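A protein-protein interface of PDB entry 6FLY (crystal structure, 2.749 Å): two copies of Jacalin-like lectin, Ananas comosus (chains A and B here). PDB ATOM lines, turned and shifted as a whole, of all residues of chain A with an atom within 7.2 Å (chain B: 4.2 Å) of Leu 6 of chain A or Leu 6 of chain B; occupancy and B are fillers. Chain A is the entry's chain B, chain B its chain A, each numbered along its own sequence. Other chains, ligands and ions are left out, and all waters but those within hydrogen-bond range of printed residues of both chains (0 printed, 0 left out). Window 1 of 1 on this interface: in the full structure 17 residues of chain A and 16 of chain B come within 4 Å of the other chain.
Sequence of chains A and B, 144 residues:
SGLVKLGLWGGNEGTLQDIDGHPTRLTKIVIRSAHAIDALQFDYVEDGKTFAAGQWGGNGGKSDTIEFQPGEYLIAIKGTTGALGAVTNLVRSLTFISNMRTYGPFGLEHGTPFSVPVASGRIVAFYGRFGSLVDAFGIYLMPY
The backbone carbonyl oxygen (O) of Ser 120 of chain A sits at hydrogen-bond distance from the backbone NH (N) of Lys 5 of chain B, at 2.9 Å.
The backbone NH (N) of Gly 7 of chain B is in hydrogen-bond range of the backbone carbonyl oxygen (O) of Pro 117 of chain A, 2.8 Å away.
The backbone carbonyl oxygen of Lys 5 of chain B sits at hydrogen-bond distance from the backbone NH of Ala 119 of chain A (2.7 Å).
The backbone carbonyl oxygen of Pro 117 of chain B is in hydrogen-bond range of the backbone NH of Gly 7 of chain A, at 2.9 Å.
NE1 of Trp 9 of chain B sits at hydrogen-bond distance from O of Ser 115 of chain A (3.2 Å).
O of Val 4 of chain A lies within hydrogen-bond range of N of Leu 141 of chain A (2.8 Å).
The backbone NH (N) of Leu 141 of chain B lies within hydrogen-bond range of the backbone carbonyl oxygen (O) of Val 4 of chain B.
O of Tyr 127 of chain B is in hydrogen-bond range of N of Gly 138 of chain B (2.9 Å).
The backbone carbonyl oxygen (O) of Ile 139 of chain B lies within hydrogen-bond range of the backbone NH (N) of Leu 6 of chain B (2.9 Å).
The backbone carbonyl oxygen of Ile 139 of chain A sits at hydrogen-bond distance from the backbone NH of Leu 6 of chain A (2.9 Å).
The backbone carbonyl oxygen (O) of Trp 9 of chain A is in hydrogen-bond range of the backbone NH (N) of Phe 137 of chain A.
Val 4 of chain A touches Val 4 of chain B.
CD1 of Leu 6 of chain A touches CD1 of Leu 6 of chain B, 3.6 Å away.
CA of Leu 6 of chain A touches O of Pro 117 of chain B, 3.4 Å away.
Pro 117 of chain B touches Leu 8 of chain A.
NE1 of Trp 9 of chain A touches CD of Pro 117 of chain B, 3.6 Å away.
Pro 117 of chain A touches Leu 6 of chain B.
CD of Pro 117 of chain A touches CZ2 of Trp 9 of chain B, 3.6 Å away.
Val 118 of chain A touches Lys 5 of chain B.
N of Ala 119 of chain A touches O of Gly 7 of chain B, at 3.7 Å.
Leu 141 of chain A touches Leu 6 of chain B.
Printed residues of chain B within 4 Å of Leu 6 of chain A: Leu 6 and Pro 117.
Of chain A, only Leu 6 (3.6 Å), Pro 117 (3.4 Å) and Leu 141 (3.98 Å) come within 4 Å of Leu 6 of chain B.
Of the printed residues of chain B, Ala 119 of chain A touches Lys 5, Gly 7 and Tyr 127.
Printed residues of chain B within 4 Å of Ser 120 of chain A: Val 4 (3.6 Å) and Lys 5 (2.9 Å).
The nearest printed residue of chain B that does not touch Leu 6 of chain A is Leu 141 of chain B (4.2 Å).
The nearest printed residue of chain B that does not touch Ser 115 of chain A is Val 116 of chain B (5.4 Å).
Hydrophobic or aromatic side chains of chain B that line the printed part of chain A: Val 4, Leu 6, Trp 9, Pro 117 and Tyr 127.
Hydrophobic or aromatic side chains of chain A that line the printed part of chain B: Val 4, Leu 6, Trp 9, Pro 117, Ala 119 and Leu 141.
Among the printed residues, 17 pairs touch across the chains.
Val 4 of chain B touches its own counterpart, Val 4 of chain A.
Leu 6 of chain A touches Pro 117 of chain B, and with the chains exchanged Pro 117 of chain A touches Leu 6 of chain B.
Gly 7 of chain A touches Pro 117 of chain B, and with the chains exchanged Pro 117 of chain A touches Gly 7 of chain B.
Leu 141 of chain A touches Leu 6 of chain B, but with the chains exchanged Leu 6 of chain A does not touch Leu 141 of chain B (4.2 Å).
Positions printed for both chains: 4, 5, 6, 7, 9, 116, 117, 127, 138, 139 and 141.
Of the 17 pairs that touch across the chains among the printed residues, 8 have their exchanged pair printed and touching as well.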
ATOM      1  N   LEU A   3     -25.873  -5.839 -10.154  1.00  0.00           N
ATOM      2  CA  LEU A   3     -25.338  -5.720  -8.807  1.00  0.00           C
ATOM      3  C   LEU A   3     -25.618  -4.325  -8.257  1.00  0.00           C
ATOM      4  O   LEU A   3     -25.610  -3.336  -8.998  1.00  0.00           O
ATOM      5  CB  LEU A   3     -23.843  -6.040  -8.751  1.00  0.00           C
ATOM      6  CG  LEU A   3     -23.471  -7.437  -9.250  1.00  0.00           C
ATOM      7  CD1 LEU A   3     -21.959  -7.607  -9.276  1.00  0.00           C
ATOM      8  CD2 LEU A   3     -24.124  -8.537  -8.400  1.00  0.00           C
ATOM      9  N   VAL A   4     -25.866  -4.253  -6.953  1.00  0.00           N
ATOM     10  CA  VAL A   4     -25.892  -2.970  -6.255  1.00  0.00           C
ATOM     11  C   VAL A   4     -24.461  -2.602  -5.893  1.00  0.00           C
ATOM     12  O   VAL A   4     -23.721  -3.416  -5.334  1.00  0.00           O
ATOM     13  CB  VAL A   4     -26.775  -3.052  -5.001  1.00  0.00           C
ATOM     14  CG1 VAL A   4     -26.638  -1.793  -4.151  1.00  0.00           C
ATOM     15  CG2 VAL A   4     -28.222  -3.270  -5.378  1.00  0.00           C
ATOM     16  N   LYS A   5     -24.067  -1.375  -6.217  1.00  0.00           N
ATOM     17  CA  LYS A   5     -22.696  -0.904  -6.027  1.00  0.00           C
ATOM     18  C   LYS A   5     -22.692   0.240  -5.017  1.00  0.00           C
ATOM     19  O   LYS A   5     -23.248   1.312  -5.281  1.00  0.00           O
ATOM     20  CB  LYS A   5     -22.112  -0.485  -7.375  1.00  0.00           C
ATOM     21  CG  LYS A   5     -20.627  -0.185  -7.399  1.00  0.00           C
ATOM     22  CD  LYS A   5     -20.232   0.210  -8.815  1.00  0.00           C
ATOM     23  CE  LYS A   5     -18.746   0.446  -8.973  1.00  0.00           C
ATOM     24  NZ  LYS A   5     -18.402   0.692 -10.403  1.00  0.00           N
ATOM     25  N   LEU A   6     -22.070   0.010  -3.861  1.00  0.00           N
ATOM     26  CA  LEU A   6     -21.980   1.000  -2.794  1.00  0.00           C
ATOM     27  C   LEU A   6     -20.576   1.583  -2.731  1.00  0.00           C
ATOM     28  O   LEU A   6     -19.585   0.863  -2.893  1.00  0.00           O
ATOM     29  CB  LEU A   6     -22.335   0.381  -1.439  1.00  0.00           C
ATOM     30  CG  LEU A   6     -23.687  -0.323  -1.360  1.00  0.00           C
ATOM     31  CD1 LEU A   6     -23.905  -0.907   0.021  1.00  0.00           C
ATOM     32  CD2 LEU A   6     -24.797   0.658  -1.703  1.00  0.00           C
ATOM     33  N   GLY A   7     -20.497   2.891  -2.512  1.00  0.00           N
ATOM     34  CA  GLY A   7     -19.215   3.563  -2.403  1.00  0.00           C
ATOM     35  C   GLY A   7     -19.264   4.941  -3.026  1.00  0.00           C
ATOM     36  O   GLY A   7     -20.296   5.316  -3.587  1.00  0.00           O
ATOM     37  N   LEU A   8     -18.178   5.709  -2.946  1.00  0.00           N
ATOM     38  CA  LEU A   8     -16.931   5.323  -2.280  1.00  0.00           C
ATOM     39  C   LEU A   8     -16.848   5.863  -0.857  1.00  0.00           C
ATOM     40  O   LEU A   8     -17.347   6.948  -0.561  1.00  0.00           O
ATOM     41  CB  LEU A   8     -15.718   5.814  -3.070  1.00  0.00           C
ATOM     42  CG  LEU A   8     -15.416   5.123  -4.402  1.00  0.00           C
ATOM     43  CD1 LEU A   8     -14.433   5.942  -5.218  1.00  0.00           C
ATOM     44  CD2 LEU A   8     -14.866   3.732  -4.145  1.00  0.00           C
ATOM     45  N   TRP A   9     -16.234   5.083   0.025  1.00  0.00           N
ATOM     46  CA  TRP A   9     -15.807   5.568   1.329  1.00  0.00           C
ATOM     47  C   TRP A   9     -14.324   5.908   1.257  1.00  0.00           C
ATOM     48  O   TRP A   9     -13.509   5.062   0.871  1.00  0.00           O
ATOM     49  CB  TRP A   9     -16.043   4.533   2.431  1.00  0.00           C
ATOM     50  CG  TRP A   9     -17.481   4.255   2.729  1.00  0.00           C
ATOM     51  CD1 TRP A   9     -18.294   4.959   3.571  1.00  0.00           C
ATOM     52  CD2 TRP A   9     -18.267   3.163   2.234  1.00  0.00           C
ATOM     53  NE1 TRP A   9     -19.546   4.389   3.607  1.00  0.00           N
ATOM     54  CE2 TRP A   9     -19.552   3.283   2.799  1.00  0.00           C
ATOM     55  CE3 TRP A   9     -18.010   2.102   1.362  1.00  0.00           C
ATOM     56  CZ2 TRP A   9     -20.579   2.383   2.518  1.00  0.00           C
ATOM     57  CZ3 TRP A   9     -19.029   1.210   1.082  1.00  0.00           C
ATOM     58  CH2 TRP A   9     -20.299   1.357   1.658  1.00  0.00           C
ATOM     59  N   SER A 115     -20.088   1.513   8.202  1.00  0.00           N
ATOM     60  CA  SER A 115     -20.519   0.145   8.439  1.00  0.00           C
ATOM     61  C   SER A 115     -21.605  -0.236   7.449  1.00  0.00           C
ATOM     62  O   SER A 115     -22.506   0.552   7.155  1.00  0.00           O
ATOM     63  CB  SER A 115     -21.032  -0.043   9.871  1.00  0.00           C
ATOM     64  OG  SER A 115     -22.020   0.921  10.198  1.00  0.00           O
ATOM     65  N   VAL A 116     -21.505  -1.462   6.953  1.00  0.00           N
ATOM     66  CA  VAL A 116     -22.441  -2.034   5.996  1.00  0.00           C
ATOM     67  C   VAL A 116     -22.906  -3.386   6.526  1.00  0.00           C
ATOM     68  O   VAL A 116     -22.279  -4.418   6.229  1.00  0.00           O
ATOM     69  CB  VAL A 116     -21.793  -2.167   4.609  1.00  0.00           C
ATOM     70  CG1 VAL A 116     -22.814  -2.639   3.586  1.00  0.00           C
ATOM     71  CG2 VAL A 116     -21.183  -0.837   4.184  1.00  0.00           C
ATOM     72  N   PRO A 117     -23.917  -3.419   7.397  1.00  0.00           N
ATOM     73  CA  PRO A 117     -24.537  -4.698   7.764  1.00  0.00           C
ATOM     74  C   PRO A 117     -25.512  -5.132   6.678  1.00  0.00           C
ATOM     75  O   PRO A 117     -26.341  -4.341   6.221  1.00  0.00           O
ATOM     76  CB  PRO A 117     -25.252  -4.384   9.081  1.00  0.00           C
ATOM     77  CG  PRO A 117     -25.580  -2.937   8.995  1.00  0.00           C
ATOM     78  CD  PRO A 117     -24.516  -2.286   8.128  1.00  0.00           C
ATOM     79  N   VAL A 118     -25.429  -6.397   6.285  1.00  0.00           N
ATOM     80  CA  VAL A 118     -26.230  -6.941   5.196  1.00  0.00           C
ATOM     81  C   VAL A 118     -27.285  -7.845   5.820  1.00  0.00           C
ATOM     82  O   VAL A 118     -26.961  -8.912   6.357  1.00  0.00           O
ATOM     83  CB  VAL A 118     -25.365  -7.698   4.178  1.00  0.00           C
ATOM     84  CG1 VAL A 118     -26.215  -8.204   3.017  1.00  0.00           C
ATOM     85  CG2 VAL A 118     -24.235  -6.807   3.675  1.00  0.00           C
ATOM     86  N   ALA A 119     -28.549  -7.416   5.757  1.00  0.00           N
ATOM     87  CA  ALA A 119     -29.642  -8.248   6.247  1.00  0.00           C
ATOM     88  C   ALA A 119     -30.047  -9.304   5.228  1.00  0.00           C
ATOM     89  O   ALA A 119     -30.382 -10.434   5.603  1.00  0.00           O
ATOM     90  CB  ALA A 119     -30.844  -7.376   6.606  1.00  0.00           C
ATOM     91  N   SER A 120     -30.031  -8.956   3.944  1.00  0.00           N
ATOM     92  CA  SER A 120     -30.318  -9.908   2.877  1.00  0.00           C
ATOM     93  C   SER A 120     -29.480  -9.525   1.670  1.00  0.00           C
ATOM     94  O   SER A 120     -29.646  -8.430   1.123  1.00  0.00           O
ATOM     95  CB  SER A 120     -31.807  -9.933   2.524  1.00  0.00           C
ATOM     96  OG  SER A 120     -32.087 -10.951   1.576  1.00  0.00           O
ATOM     97  N   GLY A 121     -28.606 -10.419   1.252  1.00  0.00           N
ATOM     98  CA  GLY A 121     -27.765 -10.178   0.095  1.00  0.00           C
ATOM     99  C   GLY A 121     -26.425 -10.862   0.260  1.00  0.00           C
ATOM    100  O   GLY A 121     -26.137 -11.488   1.276  1.00  0.00           O
ATOM    101  N   TYR A 127     -14.402  -2.525  -5.187  1.00  0.00           N
ATOM    102  CA  TYR A 127     -13.647  -1.611  -6.042  1.00  0.00           C
ATOM    103  C   TYR A 127     -13.080  -0.504  -5.163  1.00  0.00           C
ATOM    104  O   TYR A 127     -13.277  -0.507  -3.947  1.00  0.00           O
ATOM    105  CB  TYR A 127     -14.519  -1.080  -7.187  1.00  0.00           C
ATOM    106  CG  TYR A 127     -15.526  -0.021  -6.797  1.00  0.00           C
ATOM    107  CD1 TYR A 127     -16.611  -0.330  -5.987  1.00  0.00           C
ATOM    108  CD2 TYR A 127     -15.397   1.286  -7.246  1.00  0.00           C
ATOM    109  CE1 TYR A 127     -17.542   0.632  -5.640  1.00  0.00           C
ATOM    110  CE2 TYR A 127     -16.319   2.255  -6.900  1.00  0.00           C
ATOM    111  CZ  TYR A 127     -17.388   1.924  -6.095  1.00  0.00           C
ATOM    112  OH  TYR A 127     -18.308   2.886  -5.749  1.00  0.00           O
ATOM    113  N   PHE A 137     -12.737   2.972  -0.977  1.00  0.00           N
ATOM    114  CA  PHE A 137     -13.207   1.593  -0.931  1.00  0.00           C
ATOM    115  C   PHE A 137     -14.697   1.526  -1.253  1.00  0.00           C
ATOM    116  O   PHE A 137     -15.469   2.409  -0.861  1.00  0.00           O
ATOM    117  CB  PHE A 137     -12.914   1.015   0.469  1.00  0.00           C
ATOM    118  CG  PHE A 137     -13.497  -0.347   0.718  1.00  0.00           C
ATOM    119  CD1 PHE A 137     -12.877  -1.476   0.217  1.00  0.00           C
ATOM    120  CD2 PHE A 137     -14.627  -0.504   1.508  1.00  0.00           C
ATOM    121  CE1 PHE A 137     -13.391  -2.733   0.460  1.00  0.00           C
ATOM    122  CE2 PHE A 137     -15.145  -1.764   1.757  1.00  0.00           C
ATOM    123  CZ  PHE A 137     -14.524  -2.879   1.233  1.00  0.00           C
ATOM    124  N   GLY A 138     -15.094   0.466  -1.972  1.00  0.00           N
ATOM    125  CA  GLY A 138     -16.487   0.224  -2.299  1.00  0.00           C
ATOM    126  C   GLY A 138     -16.771  -1.255  -2.464  1.00  0.00           C
ATOM    127  O   GLY A 138     -15.860  -2.073  -2.633  1.00  0.00           O
ATOM    128  N   ILE A 139     -18.071  -1.569  -2.528  1.00  0.00           N
ATOM    129  CA  ILE A 139     -18.582  -2.930  -2.380  1.00  0.00           C
ATOM    130  C   ILE A 139     -19.620  -3.218  -3.457  1.00  0.00           C
ATOM    131  O   ILE A 139     -20.435  -2.353  -3.792  1.00  0.00           O
ATOM    132  CB  ILE A 139     -19.220  -3.128  -0.987  1.00  0.00           C
ATOM    133  CG1 ILE A 139     -18.221  -2.796   0.133  1.00  0.00           C
ATOM    134  CG2 ILE A 139     -19.768  -4.551  -0.829  1.00  0.00           C
ATOM    135  CD1 ILE A 139     -18.875  -2.608   1.485  1.00  0.00           C
ATOM    136  N   TYR A 140     -19.582  -4.431  -4.001  1.00  0.00           N
ATOM    137  CA  TYR A 140     -20.628  -4.950  -4.874  1.00  0.00           C
ATOM    138  C   TYR A 140     -21.455  -5.965  -4.099  1.00  0.00           C
ATOM    139  O   TYR A 140     -20.898  -6.867  -3.462  1.00  0.00           O
ATOM    140  CB  TYR A 140     -20.060  -5.622  -6.128  1.00  0.00           C
ATOM    141  CG  TYR A 140     -19.536  -4.688  -7.190  1.00  0.00           C
ATOM    142  CD1 TYR A 140     -20.382  -4.167  -8.162  1.00  0.00           C
ATOM    143  CD2 TYR A 140     -18.183  -4.387  -7.271  1.00  0.00           C
ATOM    144  CE1 TYR A 140     -19.900  -3.337  -9.152  1.00  0.00           C
ATOM    145  CE2 TYR A 140     -17.692  -3.558  -8.261  1.00  0.00           C
ATOM    146  CZ  TYR A 140     -18.558  -3.038  -9.202  1.00  0.00           C
ATOM    147  OH  TYR A 140     -18.083  -2.207 -10.187  1.00  0.00           O
ATOM    148  N   LEU A 141     -22.777  -5.821  -4.150  1.00  0.00           N
ATOM    149  CA  LEU A 141     -23.694  -6.747  -3.502  1.00  0.00           C
ATOM    150  C   LEU A 141     -24.678  -7.294  -4.525  1.00  0.00           C
ATOM    151  O   LEU A 141     -25.113  -6.582  -5.434  1.00  0.00           O
ATOM    152  CB  LEU A 141     -24.473  -6.086  -2.360  1.00  0.00           C
ATOM    153  CG  LEU A 141     -23.636  -5.492  -1.232  1.00  0.00           C
ATOM    154  CD1 LEU A 141     -23.498  -3.999  -1.436  1.00  0.00           C
ATOM    155  CD2 LEU A 141     -24.274  -5.777   0.115  1.00  0.00           C
ATOM    156  N   VAL B   4     -31.555  -5.927  -2.391  1.00  0.00           N
ATOM    157  CA  VAL B   4     -30.515  -5.987  -1.370  1.00  0.00           C
ATOM    158  C   VAL B   4     -31.029  -5.240  -0.145  1.00  0.00           C
ATOM    159  O   VAL B   4     -31.528  -4.115  -0.252  1.00  0.00           O
ATOM    160  CB  VAL B   4     -29.192  -5.401  -1.884  1.00  0.00           C
ATOM    161  CG1 VAL B   4     -28.196  -5.275  -0.740  1.00  0.00           C
ATOM    162  CG2 VAL B   4     -28.638  -6.289  -2.984  1.00  0.00           C
ATOM    163  N   LYS B   5     -30.925  -5.866   1.026  1.00  0.00           N
ATOM    164  CA  LYS B   5     -31.461  -5.322   2.274  1.00  0.00           C
ATOM    165  C   LYS B   5     -30.301  -5.042   3.223  1.00  0.00           C
ATOM    166  O   LYS B   5     -29.628  -5.974   3.679  1.00  0.00           O
ATOM    167  CB  LYS B   5     -32.452  -6.299   2.904  1.00  0.00           C
ATOM    168  CG  LYS B   5     -33.247  -5.768   4.091  1.00  0.00           C
ATOM    169  CD  LYS B   5     -34.169  -6.869   4.595  1.00  0.00           C
ATOM    170  CE  LYS B   5     -35.070  -6.420   5.725  1.00  0.00           C
ATOM    171  NZ  LYS B   5     -36.033  -7.495   6.085  1.00  0.00           N
ATOM    172  N   LEU B   6     -30.075  -3.767   3.529  1.00  0.00           N
ATOM    173  CA  LEU B   6     -29.000  -3.359   4.421  1.00  0.00           C
ATOM    174  C   LEU B   6     -29.572  -2.950   5.772  1.00  0.00           C
ATOM    175  O   LEU B   6     -30.609  -2.283   5.841  1.00  0.00           O
ATOM    176  CB  LEU B   6     -28.215  -2.181   3.844  1.00  0.00           C
ATOM    177  CG  LEU B   6     -27.639  -2.326   2.435  1.00  0.00           C
ATOM    178  CD1 LEU B   6     -26.910  -1.044   2.067  1.00  0.00           C
ATOM    179  CD2 LEU B   6     -26.748  -3.549   2.288  1.00  0.00           C
ATOM    180  N   GLY B   7     -28.889  -3.344   6.840  1.00  0.00           N
ATOM    181  CA  GLY B   7     -29.305  -2.996   8.184  1.00  0.00           C
ATOM    182  C   GLY B   7     -29.047  -4.122   9.160  1.00  0.00           C
ATOM    183  O   GLY B   7     -28.595  -5.189   8.750  1.00  0.00           O
ATOM    184  N   TRP B   9     -28.954  -0.447  11.420  1.00  0.00           N
ATOM    185  CA  TRP B   9     -28.194   0.554  12.154  1.00  0.00           C
ATOM    186  C   TRP B   9     -29.020   1.013  13.345  1.00  0.00           C
ATOM    187  O   TRP B   9     -30.168   1.441  13.184  1.00  0.00           O
ATOM    188  CB  TRP B   9     -27.852   1.764  11.284  1.00  0.00           C
ATOM    189  CG  TRP B   9     -26.887   1.501  10.174  1.00  0.00           C
ATOM    190  CD1 TRP B   9     -25.526   1.517  10.252  1.00  0.00           C
ATOM    191  CD2 TRP B   9     -27.209   1.227   8.806  1.00  0.00           C
ATOM    192  NE1 TRP B   9     -24.977   1.248   9.021  1.00  0.00           N
ATOM    193  CE2 TRP B   9     -25.989   1.069   8.115  1.00  0.00           C
ATOM    194  CE3 TRP B   9     -28.407   1.093   8.100  1.00  0.00           C
ATOM    195  CZ2 TRP B   9     -25.935   0.782   6.752  1.00  0.00           C
ATOM    196  CZ3 TRP B   9     -28.350   0.806   6.748  1.00  0.00           C
ATOM    197  CH2 TRP B   9     -27.124   0.652   6.090  1.00  0.00           C
ATOM    198  N   VAL B 116     -24.187   5.626   3.560  1.00  0.00           N
ATOM    199  CA  VAL B 116     -24.483   4.696   2.478  1.00  0.00           C
ATOM    200  C   VAL B 116     -24.479   5.488   1.176  1.00  0.00           C
ATOM    201  O   VAL B 116     -25.527   6.022   0.772  1.00  0.00           O
ATOM    202  CB  VAL B 116     -25.835   4.000   2.706  1.00  0.00           C
ATOM    203  CG1 VAL B 116     -26.076   2.930   1.650  1.00  0.00           C
ATOM    204  CG2 VAL B 116     -25.905   3.421   4.116  1.00  0.00           C
ATOM    205  N   PRO B 117     -23.313   5.700   0.563  1.00  0.00           N
ATOM    206  CA  PRO B 117     -23.268   6.267  -0.792  1.00  0.00           C
ATOM    207  C   PRO B 117     -23.558   5.182  -1.820  1.00  0.00           C
ATOM    208  O   PRO B 117     -22.991   4.088  -1.758  1.00  0.00           O
ATOM    209  CB  PRO B 117     -21.833   6.793  -0.909  1.00  0.00           C
ATOM    210  CG  PRO B 117     -21.044   5.907  -0.005  1.00  0.00           C
ATOM    211  CD  PRO B 117     -21.965   5.454   1.104  1.00  0.00           C
ATOM    212  N   TYR B 127     -36.880  -0.222   6.338  1.00  0.00           N
ATOM    213  CA  TYR B 127     -37.471  -0.955   7.456  1.00  0.00           C
ATOM    214  C   TYR B 127     -36.750  -0.515   8.724  1.00  0.00           C
ATOM    215  O   TYR B 127     -35.863   0.336   8.681  1.00  0.00           O
ATOM    216  CB  TYR B 127     -37.400  -2.473   7.248  1.00  0.00           C
ATOM    217  CG  TYR B 127     -36.035  -3.088   7.474  1.00  0.00           C
ATOM    218  CD1 TYR B 127     -34.973  -2.825   6.618  1.00  0.00           C
ATOM    219  CD2 TYR B 127     -35.814  -3.943   8.544  1.00  0.00           C
ATOM    220  CE1 TYR B 127     -33.730  -3.399   6.825  1.00  0.00           C
ATOM    221  CE2 TYR B 127     -34.578  -4.516   8.759  1.00  0.00           C
ATOM    222  CZ  TYR B 127     -33.537  -4.237   7.899  1.00  0.00           C
ATOM    223  OH  TYR B 127     -32.303  -4.806   8.113  1.00  0.00           O
ATOM    224  N   GLY B 138     -33.029   0.572   8.417  1.00  0.00           N
ATOM    225  CA  GLY B 138     -32.462  -0.193   7.322  1.00  0.00           C
ATOM    226  C   GLY B 138     -33.073   0.211   5.995  1.00  0.00           C
ATOM    227  O   GLY B 138     -34.129   0.850   5.943  1.00  0.00           O
ATOM    228  N   ILE B 139     -32.448  -0.272   4.915  1.00  0.00           N
ATOM    229  CA  ILE B 139     -32.670   0.229   3.562  1.00  0.00           C
ATOM    230  C   ILE B 139     -32.840  -0.938   2.600  1.00  0.00           C
ATOM    231  O   ILE B 139     -32.142  -1.952   2.706  1.00  0.00           O
ATOM    232  CB  ILE B 139     -31.488   1.104   3.080  1.00  0.00           C
ATOM    233  CG1 ILE B 139     -31.218   2.271   4.033  1.00  0.00           C
ATOM    234  CG2 ILE B 139     -31.733   1.606   1.657  1.00  0.00           C
ATOM    235  CD1 ILE B 139     -29.857   2.914   3.799  1.00  0.00           C
ATOM    236  N   LEU B 141     -32.535  -1.724  -1.462  1.00  0.00           N
ATOM    237  CA  LEU B 141     -31.988  -1.223  -2.714  1.00  0.00           C
ATOM    238  C   LEU B 141     -32.265  -2.198  -3.848  1.00  0.00           C
ATOM    239  O   LEU B 141     -32.231  -3.418  -3.665  1.00  0.00           O
ATOM    240  CB  LEU B 141     -30.488  -0.966  -2.639  1.00  0.00           C
ATOM    241  CG  LEU B 141     -30.076   0.041  -1.573  1.00  0.00           C
ATOM    242  CD1 LEU B 141     -29.614  -0.696  -0.343  1.00  0.00           C
ATOM    243  CD2 LEU B 141     -28.984   0.954  -2.101  1.00  0.00           C
